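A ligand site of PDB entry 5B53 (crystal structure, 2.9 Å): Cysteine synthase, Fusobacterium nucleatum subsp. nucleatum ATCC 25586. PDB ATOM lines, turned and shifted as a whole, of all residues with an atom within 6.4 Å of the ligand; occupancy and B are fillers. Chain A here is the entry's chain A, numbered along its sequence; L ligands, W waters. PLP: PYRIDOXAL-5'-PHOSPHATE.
The side-chain amino group (NZ) of Lys 50 is bonded to a carbon (C4A) of the ligand, 1.3 Å away.
ND2 of Asn 80 lies within hydrogen-bond range of O3 of the ligand, 2.7 Å away.
An oxygen (O2P) of the ligand lies within hydrogen-bond range of the side-chain hydroxyl of Thr 192, at 2.7 Å.
N of Thr 189 sits at hydrogen-bond distance from O1P of the ligand (2.9 Å).
O1P of the ligand sits at hydrogen-bond distance from OG1 of Thr 189, 2.5 Å away.
The backbone NH of Gly 188 sits at hydrogen-bond distance from an oxygen (O3P) of the ligand (2.8 Å).
An oxygen (O2P) of the ligand lies within hydrogen-bond range of the backbone NH of Thr 192, 2.9 Å away.
N1 of the ligand is in hydrogen-bond range of OG of Ser 276 (2.6 Å).
N of Gly 190 is in hydrogen-bond range of O3P of the ligand, at 3.1 Å.
The side-chain hydroxyl (OG1) of Thr 189 lies close to the backbone NH (N) of Gly 191, at 3.5 Å.
O of Pro 302 lies within hydrogen-bond range of N of Ile 49, at 3.1 Å.
The side-chain carboxylate (OD2) of Asp 303 lies within salt-bridge range of the side-chain amino group (NZ) of Lys 307 (3.2 Å).
The side-chain amide nitrogen of Asn 80 lies within hydrogen-bond range of the side-chain carboxylate of Asp 303, at 3.1 Å.
The backbone carbonyl oxygen of Asp 303 is in hydrogen-bond range of the backbone NH of Gly 274 (3.4 Å).
The side-chain hydroxyl (OG1) of Thr 189 is in hydrogen-bond range of the side-chain amide nitrogen (ND2) of Asn 157, at 3.1 Å.
OG of Ser 48 lies within hydrogen-bond range of N of Lys 50, at 3.0 Å.
The side-chain carboxylate (OD2) of Asp 303 lies within hydrogen-bond range of the side-chain hydroxyl (OH) of Tyr 308 (2.5 Å).
An oxygen (O3P) of the ligand lies close to the backbone carbonyl oxygen (O) of Gly 186 (3.4 Å).
Merely in contact with the ligand: Val 187 (3.4 Å), Gly 191 (3.6 Å), Glu 232 (3.5 Å), Gly 233 (3.1 Å), Ile 234 (3.6 Å), Pro 302 (3.3 Å), Asp 303 (3.4 Å) and Tyr 308 (3.5 Å).
16 residues have an atom within 4 Å of the ligand: Lys 50, Asn 80, Gly 186, Val 187, Gly 188, Thr 189, Gly 190, Gly 191, Thr 192, Glu 232, Gly 233, Ile 234, Ser 276, Pro 302, Asp 303 and Tyr 308.
The nearest printed residue that does not touch the ligand is His 161 (4.8 Å).
Water W1 lies within hydrogen-bond range of O3P of the ligand (2.5 Å), O of Gly 186 (3.0 Å) and N of Val 193 (3.3 Å).
Water W2 lies within hydrogen-bond range of a ring nitrogen (NE2) of His 161, the side-chain amide oxygen of Asn 157 and an oxygen (O2P) of the ligand.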
ATOM      1  N   SER A  48       9.432  -9.264   2.277  1.00  0.00           N
ATOM      2  CA  SER A  48       9.485 -10.588   2.798  1.00  0.00           C
ATOM      3  C   SER A  48       8.274 -10.906   3.600  1.00  0.00           C
ATOM      4  O   SER A  48       7.419 -10.055   3.899  1.00  0.00           O
ATOM      5  CB  SER A  48      10.719 -10.810   3.663  1.00  0.00           C
ATOM      6  OG  SER A  48      10.486 -10.444   5.003  1.00  0.00           O
ATOM      7  N   ILE A  49       8.239 -12.194   3.931  1.00  0.00           N
ATOM      8  CA  ILE A  49       7.165 -12.831   4.729  1.00  0.00           C
ATOM      9  C   ILE A  49       7.143 -12.296   6.167  1.00  0.00           C
ATOM     10  O   ILE A  49       6.121 -12.354   6.842  1.00  0.00           O
ATOM     11  CB  ILE A  49       7.394 -14.372   4.767  1.00  0.00           C
ATOM     12  CG1 ILE A  49       6.123 -15.080   5.233  1.00  0.00           C
ATOM     13  CG2 ILE A  49       8.567 -14.682   5.615  1.00  0.00           C
ATOM     14  CD1 ILE A  49       6.069 -16.544   4.868  1.00  0.00           C
ATOM     15  N   LYS A  50       8.270 -11.750   6.616  1.00  0.00           N
ATOM     16  CA  LYS A  50       8.358 -11.276   7.978  1.00  0.00           C
ATOM     17  C   LYS A  50       7.660  -9.931   8.117  1.00  0.00           C
ATOM     18  O   LYS A  50       7.605  -9.401   9.192  1.00  0.00           O
ATOM     19  CB  LYS A  50       9.800 -11.153   8.400  1.00  0.00           C
ATOM     20  CG  LYS A  50      10.567 -12.432   8.319  1.00  0.00           C
ATOM     21  CD  LYS A  50      10.820 -13.057   9.665  1.00  0.00           C
ATOM     22  CE  LYS A  50      11.230 -14.489   9.531  1.00  0.00           C
ATOM     23  NZ  LYS A  50      12.345 -14.623   8.548  1.00  0.00           N
ATOM     24  N   GLY A  79      18.408 -10.060   9.512  1.00  0.00           N
ATOM     25  CA  GLY A  79      17.607 -10.449   8.398  1.00  0.00           C
ATOM     26  C   GLY A  79      16.365  -9.645   8.254  1.00  0.00           C
ATOM     27  O   GLY A  79      16.262  -8.552   8.787  1.00  0.00           O
ATOM     28  N   ASN A  80      15.419 -10.231   7.537  1.00  0.00           N
ATOM     29  CA  ASN A  80      14.145  -9.613   7.305  1.00  0.00           C
ATOM     30  C   ASN A  80      13.339  -9.187   8.553  1.00  0.00           C
ATOM     31  O   ASN A  80      12.632  -8.189   8.526  1.00  0.00           O
ATOM     32  CB  ASN A  80      13.254 -10.559   6.474  1.00  0.00           C
ATOM     33  CG  ASN A  80      13.849 -10.919   5.153  1.00  0.00           C
ATOM     34  OD1 ASN A  80      14.190 -10.066   4.385  1.00  0.00           O
ATOM     35  ND2 ASN A  80      13.946 -12.181   4.869  1.00  0.00           N
ATOM     36  N   THR A  81      13.382  -9.964   9.615  1.00  0.00           N
ATOM     37  CA  THR A  81      12.798  -9.502  10.901  1.00  0.00           C
ATOM     38  C   THR A  81      13.255  -8.105  11.346  1.00  0.00           C
ATOM     39  O   THR A  81      12.443  -7.259  11.660  1.00  0.00           O
ATOM     40  CB  THR A  81      13.183 -10.434  12.025  1.00  0.00           C
ATOM     41  OG1 THR A  81      12.431 -11.626  11.898  1.00  0.00           O
ATOM     42  CG2 THR A  81      12.927  -9.815  13.381  1.00  0.00           C
ATOM     43  N   GLN A 151      11.423 -13.087  18.783  1.00  0.00           N
ATOM     44  CA  GLN A 151      10.913 -13.671  17.572  1.00  0.00           C
ATOM     45  C   GLN A 151      11.015 -15.152  17.577  1.00  0.00           C
ATOM     46  O   GLN A 151      10.277 -15.791  16.822  1.00  0.00           O
ATOM     47  CB  GLN A 151      11.655 -13.138  16.345  1.00  0.00           C
ATOM     48  CG  GLN A 151      13.155 -13.408  16.346  1.00  0.00           C
ATOM     49  CD  GLN A 151      13.838 -13.063  15.031  1.00  0.00           C
ATOM     50  OE1 GLN A 151      15.033 -12.732  15.009  1.00  0.00           O
ATOM     51  NE2 GLN A 151      13.096 -13.167  13.919  1.00  0.00           N
ATOM     52  N   ASN A 157       3.929 -14.680  16.573  1.00  0.00           N
ATOM     53  CA  ASN A 157       4.661 -14.897  15.320  1.00  0.00           C
ATOM     54  C   ASN A 157       3.911 -15.903  14.511  1.00  0.00           C
ATOM     55  O   ASN A 157       3.219 -15.531  13.577  1.00  0.00           O
ATOM     56  CB  ASN A 157       6.091 -15.383  15.688  1.00  0.00           C
ATOM     57  CG  ASN A 157       6.974 -15.762  14.505  1.00  0.00           C
ATOM     58  OD1 ASN A 157       6.511 -15.867  13.375  1.00  0.00           O
ATOM     59  ND2 ASN A 157       8.260 -16.027  14.795  1.00  0.00           N
ATOM     60  N   HIS A 161       0.997 -16.198  11.055  1.00  0.00           N
ATOM     61  CA  HIS A 161       0.922 -17.029   9.851  1.00  0.00           C
ATOM     62  C   HIS A 161      -0.304 -17.935   9.837  1.00  0.00           C
ATOM     63  O   HIS A 161      -0.839 -18.185   8.784  1.00  0.00           O
ATOM     64  CB  HIS A 161       2.217 -17.774   9.639  1.00  0.00           C
ATOM     65  CG  HIS A 161       3.385 -16.862   9.497  1.00  0.00           C
ATOM     66  ND1 HIS A 161       3.356 -15.747   8.679  1.00  0.00           N
ATOM     67  CD2 HIS A 161       4.605 -16.865  10.093  1.00  0.00           C
ATOM     68  CE1 HIS A 161       4.527 -15.129   8.746  1.00  0.00           C
ATOM     69  NE2 HIS A 161       5.299 -15.782   9.594  1.00  0.00           N
ATOM     70  N   ALA A 185       8.567 -26.024   5.124  1.00  0.00           N
ATOM     71  CA  ALA A 185       9.171 -24.680   5.292  1.00  0.00           C
ATOM     72  C   ALA A 185      10.414 -24.784   6.127  1.00  0.00           C
ATOM     73  O   ALA A 185      10.370 -25.427   7.166  1.00  0.00           O
ATOM     74  CB  ALA A 185       8.218 -23.746   5.977  1.00  0.00           C
ATOM     75  N   GLY A 186      11.505 -24.140   5.700  1.00  0.00           N
ATOM     76  CA  GLY A 186      12.710 -24.034   6.501  1.00  0.00           C
ATOM     77  C   GLY A 186      12.421 -23.205   7.738  1.00  0.00           C
ATOM     78  O   GLY A 186      11.631 -22.240   7.725  1.00  0.00           O
ATOM     79  N   VAL A 187      13.085 -23.580   8.819  1.00  0.00           N
ATOM     80  CA  VAL A 187      12.852 -23.020  10.134  1.00  0.00           C
ATOM     81  C   VAL A 187      13.973 -22.098  10.664  1.00  0.00           C
ATOM     82  O   VAL A 187      15.078 -22.548  11.034  1.00  0.00           O
ATOM     83  CB  VAL A 187      12.690 -24.170  11.159  1.00  0.00           C
ATOM     84  CG1 VAL A 187      12.936 -23.684  12.616  1.00  0.00           C
ATOM     85  CG2 VAL A 187      11.340 -24.859  10.964  1.00  0.00           C
ATOM     86  N   GLY A 188      13.664 -20.822  10.733  1.00  0.00           N
ATOM     87  CA  GLY A 188      14.458 -19.884  11.527  1.00  0.00           C
ATOM     88  C   GLY A 188      13.843 -19.744  12.913  1.00  0.00           C
ATOM     89  O   GLY A 188      14.400 -20.250  13.871  1.00  0.00           O
ATOM     90  N   THR A 189      12.724 -19.040  12.983  1.00  0.00           N
ATOM     91  CA  THR A 189      11.922 -19.003  14.197  1.00  0.00           C
ATOM     92  C   THR A 189      10.916 -20.150  14.373  1.00  0.00           C
ATOM     93  O   THR A 189      10.597 -20.547  15.504  1.00  0.00           O
ATOM     94  CB  THR A 189      11.152 -17.710  14.316  1.00  0.00           C
ATOM     95  OG1 THR A 189      10.421 -17.510  13.120  1.00  0.00           O
ATOM     96  CG2 THR A 189      12.089 -16.552  14.546  1.00  0.00           C
ATOM     97  N   GLY A 190      10.411 -20.696  13.265  1.00  0.00           N
ATOM     98  CA  GLY A 190       9.440 -21.800  13.322  1.00  0.00           C
ATOM     99  C   GLY A 190       8.064 -21.240  13.145  1.00  0.00           C
ATOM    100  O   GLY A 190       7.127 -21.985  12.951  1.00  0.00           O
ATOM    101  N   GLY A 191       7.943 -19.918  13.183  1.00  0.00           N
ATOM    102  CA  GLY A 191       6.674 -19.286  12.968  1.00  0.00           C
ATOM    103  C   GLY A 191       5.937 -19.742  11.713  1.00  0.00           C
ATOM    104  O   GLY A 191       4.773 -20.113  11.784  1.00  0.00           O
ATOM    105  N   THR A 192       6.571 -19.714  10.558  1.00  0.00           N
ATOM    106  CA  THR A 192       5.910 -20.094   9.326  1.00  0.00           C
ATOM    107  C   THR A 192       5.283 -21.516   9.386  1.00  0.00           C
ATOM    108  O   THR A 192       4.084 -21.728   9.196  1.00  0.00           O
ATOM    109  CB  THR A 192       6.972 -20.100   8.251  1.00  0.00           C
ATOM    110  OG1 THR A 192       7.465 -18.767   8.084  1.00  0.00           O
ATOM    111  CG2 THR A 192       6.426 -20.584   6.949  1.00  0.00           C
ATOM    112  N   VAL A 193       6.132 -22.483   9.670  1.00  0.00           N
ATOM    113  CA  VAL A 193       5.788 -23.893   9.580  1.00  0.00           C
ATOM    114  C   VAL A 193       4.772 -24.284  10.670  1.00  0.00           C
ATOM    115  O   VAL A 193       3.903 -25.159  10.411  1.00  0.00           O
ATOM    116  CB  VAL A 193       7.068 -24.746   9.660  1.00  0.00           C
ATOM    117  CG1 VAL A 193       7.606 -24.780  11.057  1.00  0.00           C
ATOM    118  CG2 VAL A 193       6.811 -26.127   9.163  1.00  0.00           C
ATOM    119  N   GLU A 232      20.430 -18.174   4.530  1.00  0.00           N
ATOM    120  CA  GLU A 232      20.004 -17.070   5.415  1.00  0.00           C
ATOM    121  C   GLU A 232      18.521 -16.995   5.684  1.00  0.00           C
ATOM    122  O   GLU A 232      17.731 -16.926   4.709  1.00  0.00           O
ATOM    123  CB  GLU A 232      20.226 -15.734   4.765  1.00  0.00           C
ATOM    124  CG  GLU A 232      21.640 -15.273   4.770  1.00  0.00           C
ATOM    125  CD  GLU A 232      21.742 -13.778   4.618  1.00  0.00           C
ATOM    126  OE1 GLU A 232      20.960 -13.005   5.247  1.00  0.00           O
ATOM    127  OE2 GLU A 232      22.648 -13.412   3.825  1.00  0.00           O
ATOM    128  N   GLY A 233      18.160 -16.909   6.973  1.00  0.00           N
ATOM    129  CA  GLY A 233      16.796 -16.860   7.368  1.00  0.00           C
ATOM    130  C   GLY A 233      16.420 -18.046   8.186  1.00  0.00           C
ATOM    131  O   GLY A 233      15.415 -18.008   8.871  1.00  0.00           O
ATOM    132  N   ILE A 234      17.211 -19.115   8.118  1.00  0.00           N
ATOM    133  CA  ILE A 234      16.873 -20.327   8.810  1.00  0.00           C
ATOM    134  C   ILE A 234      18.031 -20.894   9.555  1.00  0.00           C
ATOM    135  O   ILE A 234      19.165 -20.551   9.289  1.00  0.00           O
ATOM    136  CB  ILE A 234      16.395 -21.477   7.884  1.00  0.00           C
ATOM    137  CG1 ILE A 234      17.565 -22.177   7.157  1.00  0.00           C
ATOM    138  CG2 ILE A 234      15.404 -20.961   6.884  1.00  0.00           C
ATOM    139  CD1 ILE A 234      17.157 -23.446   6.406  1.00  0.00           C
ATOM    140  N   GLY A 274      15.479 -15.567  -2.785  1.00  0.00           N
ATOM    141  CA  GLY A 274      16.552 -15.838  -1.863  1.00  0.00           C
ATOM    142  C   GLY A 274      16.863 -17.301  -1.633  1.00  0.00           C
ATOM    143  O   GLY A 274      16.098 -18.187  -1.954  1.00  0.00           O
ATOM    144  N   SER A 276      17.071 -19.303   0.955  1.00  0.00           N
ATOM    145  CA  SER A 276      16.024 -20.061   1.639  1.00  0.00           C
ATOM    146  C   SER A 276      14.850 -20.605   0.663  1.00  0.00           C
ATOM    147  O   SER A 276      14.235 -21.659   0.925  1.00  0.00           O
ATOM    148  CB  SER A 276      15.488 -19.245   2.848  1.00  0.00           C
ATOM    149  OG  SER A 276      14.481 -18.307   2.507  1.00  0.00           O
ATOM    150  N   SER A 277      14.589 -19.893  -0.437  1.00  0.00           N
ATOM    151  CA  SER A 277      13.464 -20.185  -1.272  1.00  0.00           C
ATOM    152  C   SER A 277      13.837 -21.392  -2.115  1.00  0.00           C
ATOM    153  O   SER A 277      13.066 -22.343  -2.296  1.00  0.00           O
ATOM    154  CB  SER A 277      13.154 -18.962  -2.131  1.00  0.00           C
ATOM    155  OG  SER A 277      12.923 -17.802  -1.312  1.00  0.00           O
ATOM    156  N   ASN A 280      13.522 -24.406   0.346  1.00  0.00           N
ATOM    157  CA  ASN A 280      12.125 -24.828   0.340  1.00  0.00           C
ATOM    158  C   ASN A 280      11.676 -25.556  -0.912  1.00  0.00           C
ATOM    159  O   ASN A 280      10.889 -26.463  -0.844  1.00  0.00           O
ATOM    160  CB  ASN A 280      11.184 -23.632   0.552  1.00  0.00           C
ATOM    161  CG  ASN A 280      11.216 -23.131   1.985  1.00  0.00           C
ATOM    162  OD1 ASN A 280      11.955 -23.683   2.805  1.00  0.00           O
ATOM    163  ND2 ASN A 280      10.451 -22.075   2.283  1.00  0.00           N
ATOM    164  N   PRO A 302      10.296 -17.010   0.945  1.00  0.00           N
ATOM    165  CA  PRO A 302      10.265 -15.920   1.933  1.00  0.00           C
ATOM    166  C   PRO A 302      10.653 -14.530   1.407  1.00  0.00           C
ATOM    167  O   PRO A 302      10.048 -13.532   1.792  1.00  0.00           O
ATOM    168  CB  PRO A 302      11.253 -16.375   2.996  1.00  0.00           C
ATOM    169  CG  PRO A 302      11.169 -17.824   2.932  1.00  0.00           C
ATOM    170  CD  PRO A 302      11.027 -18.171   1.479  1.00  0.00           C
ATOM    171  N   ASP A 303      11.647 -14.459   0.544  1.00  0.00           N
ATOM    172  CA  ASP A 303      12.014 -13.173  -0.033  1.00  0.00           C
ATOM    173  C   ASP A 303      12.587 -13.247  -1.456  1.00  0.00           C
ATOM    174  O   ASP A 303      12.466 -14.247  -2.148  1.00  0.00           O
ATOM    175  CB  ASP A 303      12.915 -12.423   0.942  1.00  0.00           C
ATOM    176  CG  ASP A 303      14.251 -13.078   1.139  1.00  0.00           C
ATOM    177  OD1 ASP A 303      14.530 -14.101   0.479  1.00  0.00           O
ATOM    178  OD2 ASP A 303      15.022 -12.573   1.996  1.00  0.00           O
ATOM    179  N   LYS A 307      18.713  -8.648  -1.966  1.00  0.00           N
ATOM    180  CA  LYS A 307      19.688  -8.590  -0.838  1.00  0.00           C
ATOM    181  C   LYS A 307      20.895  -9.550  -0.930  1.00  0.00           C
ATOM    182  O   LYS A 307      21.893  -9.310  -0.289  1.00  0.00           O
ATOM    183  CB  LYS A 307      18.999  -8.829   0.503  1.00  0.00           C
ATOM    184  CG  LYS A 307      18.172  -7.632   1.022  1.00  0.00           C
ATOM    185  CD  LYS A 307      17.486  -7.900   2.363  1.00  0.00           C
ATOM    186  CE  LYS A 307      16.881  -9.289   2.467  1.00  0.00           C
ATOM    187  NZ  LYS A 307      15.969  -9.631   1.327  1.00  0.00           N
ATOM    188  N   TYR A 308      20.818 -10.572  -1.759  1.00  0.00           N
ATOM    189  CA  TYR A 308      21.759 -11.666  -1.752  1.00  0.00           C
ATOM    190  C   TYR A 308      22.771 -11.534  -2.868  1.00  0.00           C
ATOM    191  O   TYR A 308      23.288 -12.495  -3.444  1.00  0.00           O
ATOM    192  CB  TYR A 308      20.939 -12.924  -1.936  1.00  0.00           C
ATOM    193  CG  TYR A 308      19.968 -13.115  -0.806  1.00  0.00           C
ATOM    194  CD1 TYR A 308      18.729 -12.556  -0.854  1.00  0.00           C
ATOM    195  CD2 TYR A 308      20.319 -13.813   0.329  1.00  0.00           C
ATOM    196  CE1 TYR A 308      17.848 -12.686   0.188  1.00  0.00           C
ATOM    197  CE2 TYR A 308      19.434 -13.967   1.369  1.00  0.00           C
ATOM    198  CZ  TYR A 308      18.193 -13.388   1.292  1.00  0.00           C
ATOM    199  OH  TYR A 308      17.260 -13.541   2.285  1.00  0.00           O
HETATM  200  N1  PLP L   1      13.883 -17.464   4.839  1.00  0.00           N
HETATM  201  C2  PLP L   1      14.098 -16.116   5.088  1.00  0.00           C
HETATM  202  C2A PLP L   1      14.728 -15.199   4.078  1.00  0.00           C
HETATM  203  C3  PLP L   1      13.711 -15.607   6.322  1.00  0.00           C
HETATM  204  O3  PLP L   1      13.919 -14.280   6.620  1.00  0.00           O
HETATM  205  C4  PLP L   1      13.155 -16.468   7.276  1.00  0.00           C
HETATM  206  C4A PLP L   1      12.783 -15.890   8.615  1.00  0.00           C
HETATM  207  C5  PLP L   1      12.983 -17.815   7.019  1.00  0.00           C
HETATM  208  C6  PLP L   1      13.331 -18.291   5.781  1.00  0.00           C
HETATM  209  C5A PLP L   1      12.367 -18.730   8.029  1.00  0.00           C
HETATM  210  O4P PLP L   1      11.051 -18.352   8.548  1.00  0.00           O
HETATM  211  P   PLP L   1      10.624 -18.710  10.071  1.00  0.00           P
HETATM  212  O1P PLP L   1      11.338 -17.671  10.790  1.00  0.00           O
HETATM  213  O2P PLP L   1       9.154 -18.530  10.125  1.00  0.00           O
HETATM  214  O3P PLP L   1      11.013 -20.107  10.295  1.00  0.00           O
HETATM  215  O   HOH W   1       9.431 -22.046   9.815  1.00  0.00           O
HETATM  216  O   HOH W   2       7.737 -16.100  10.863  1.00  0.00           O
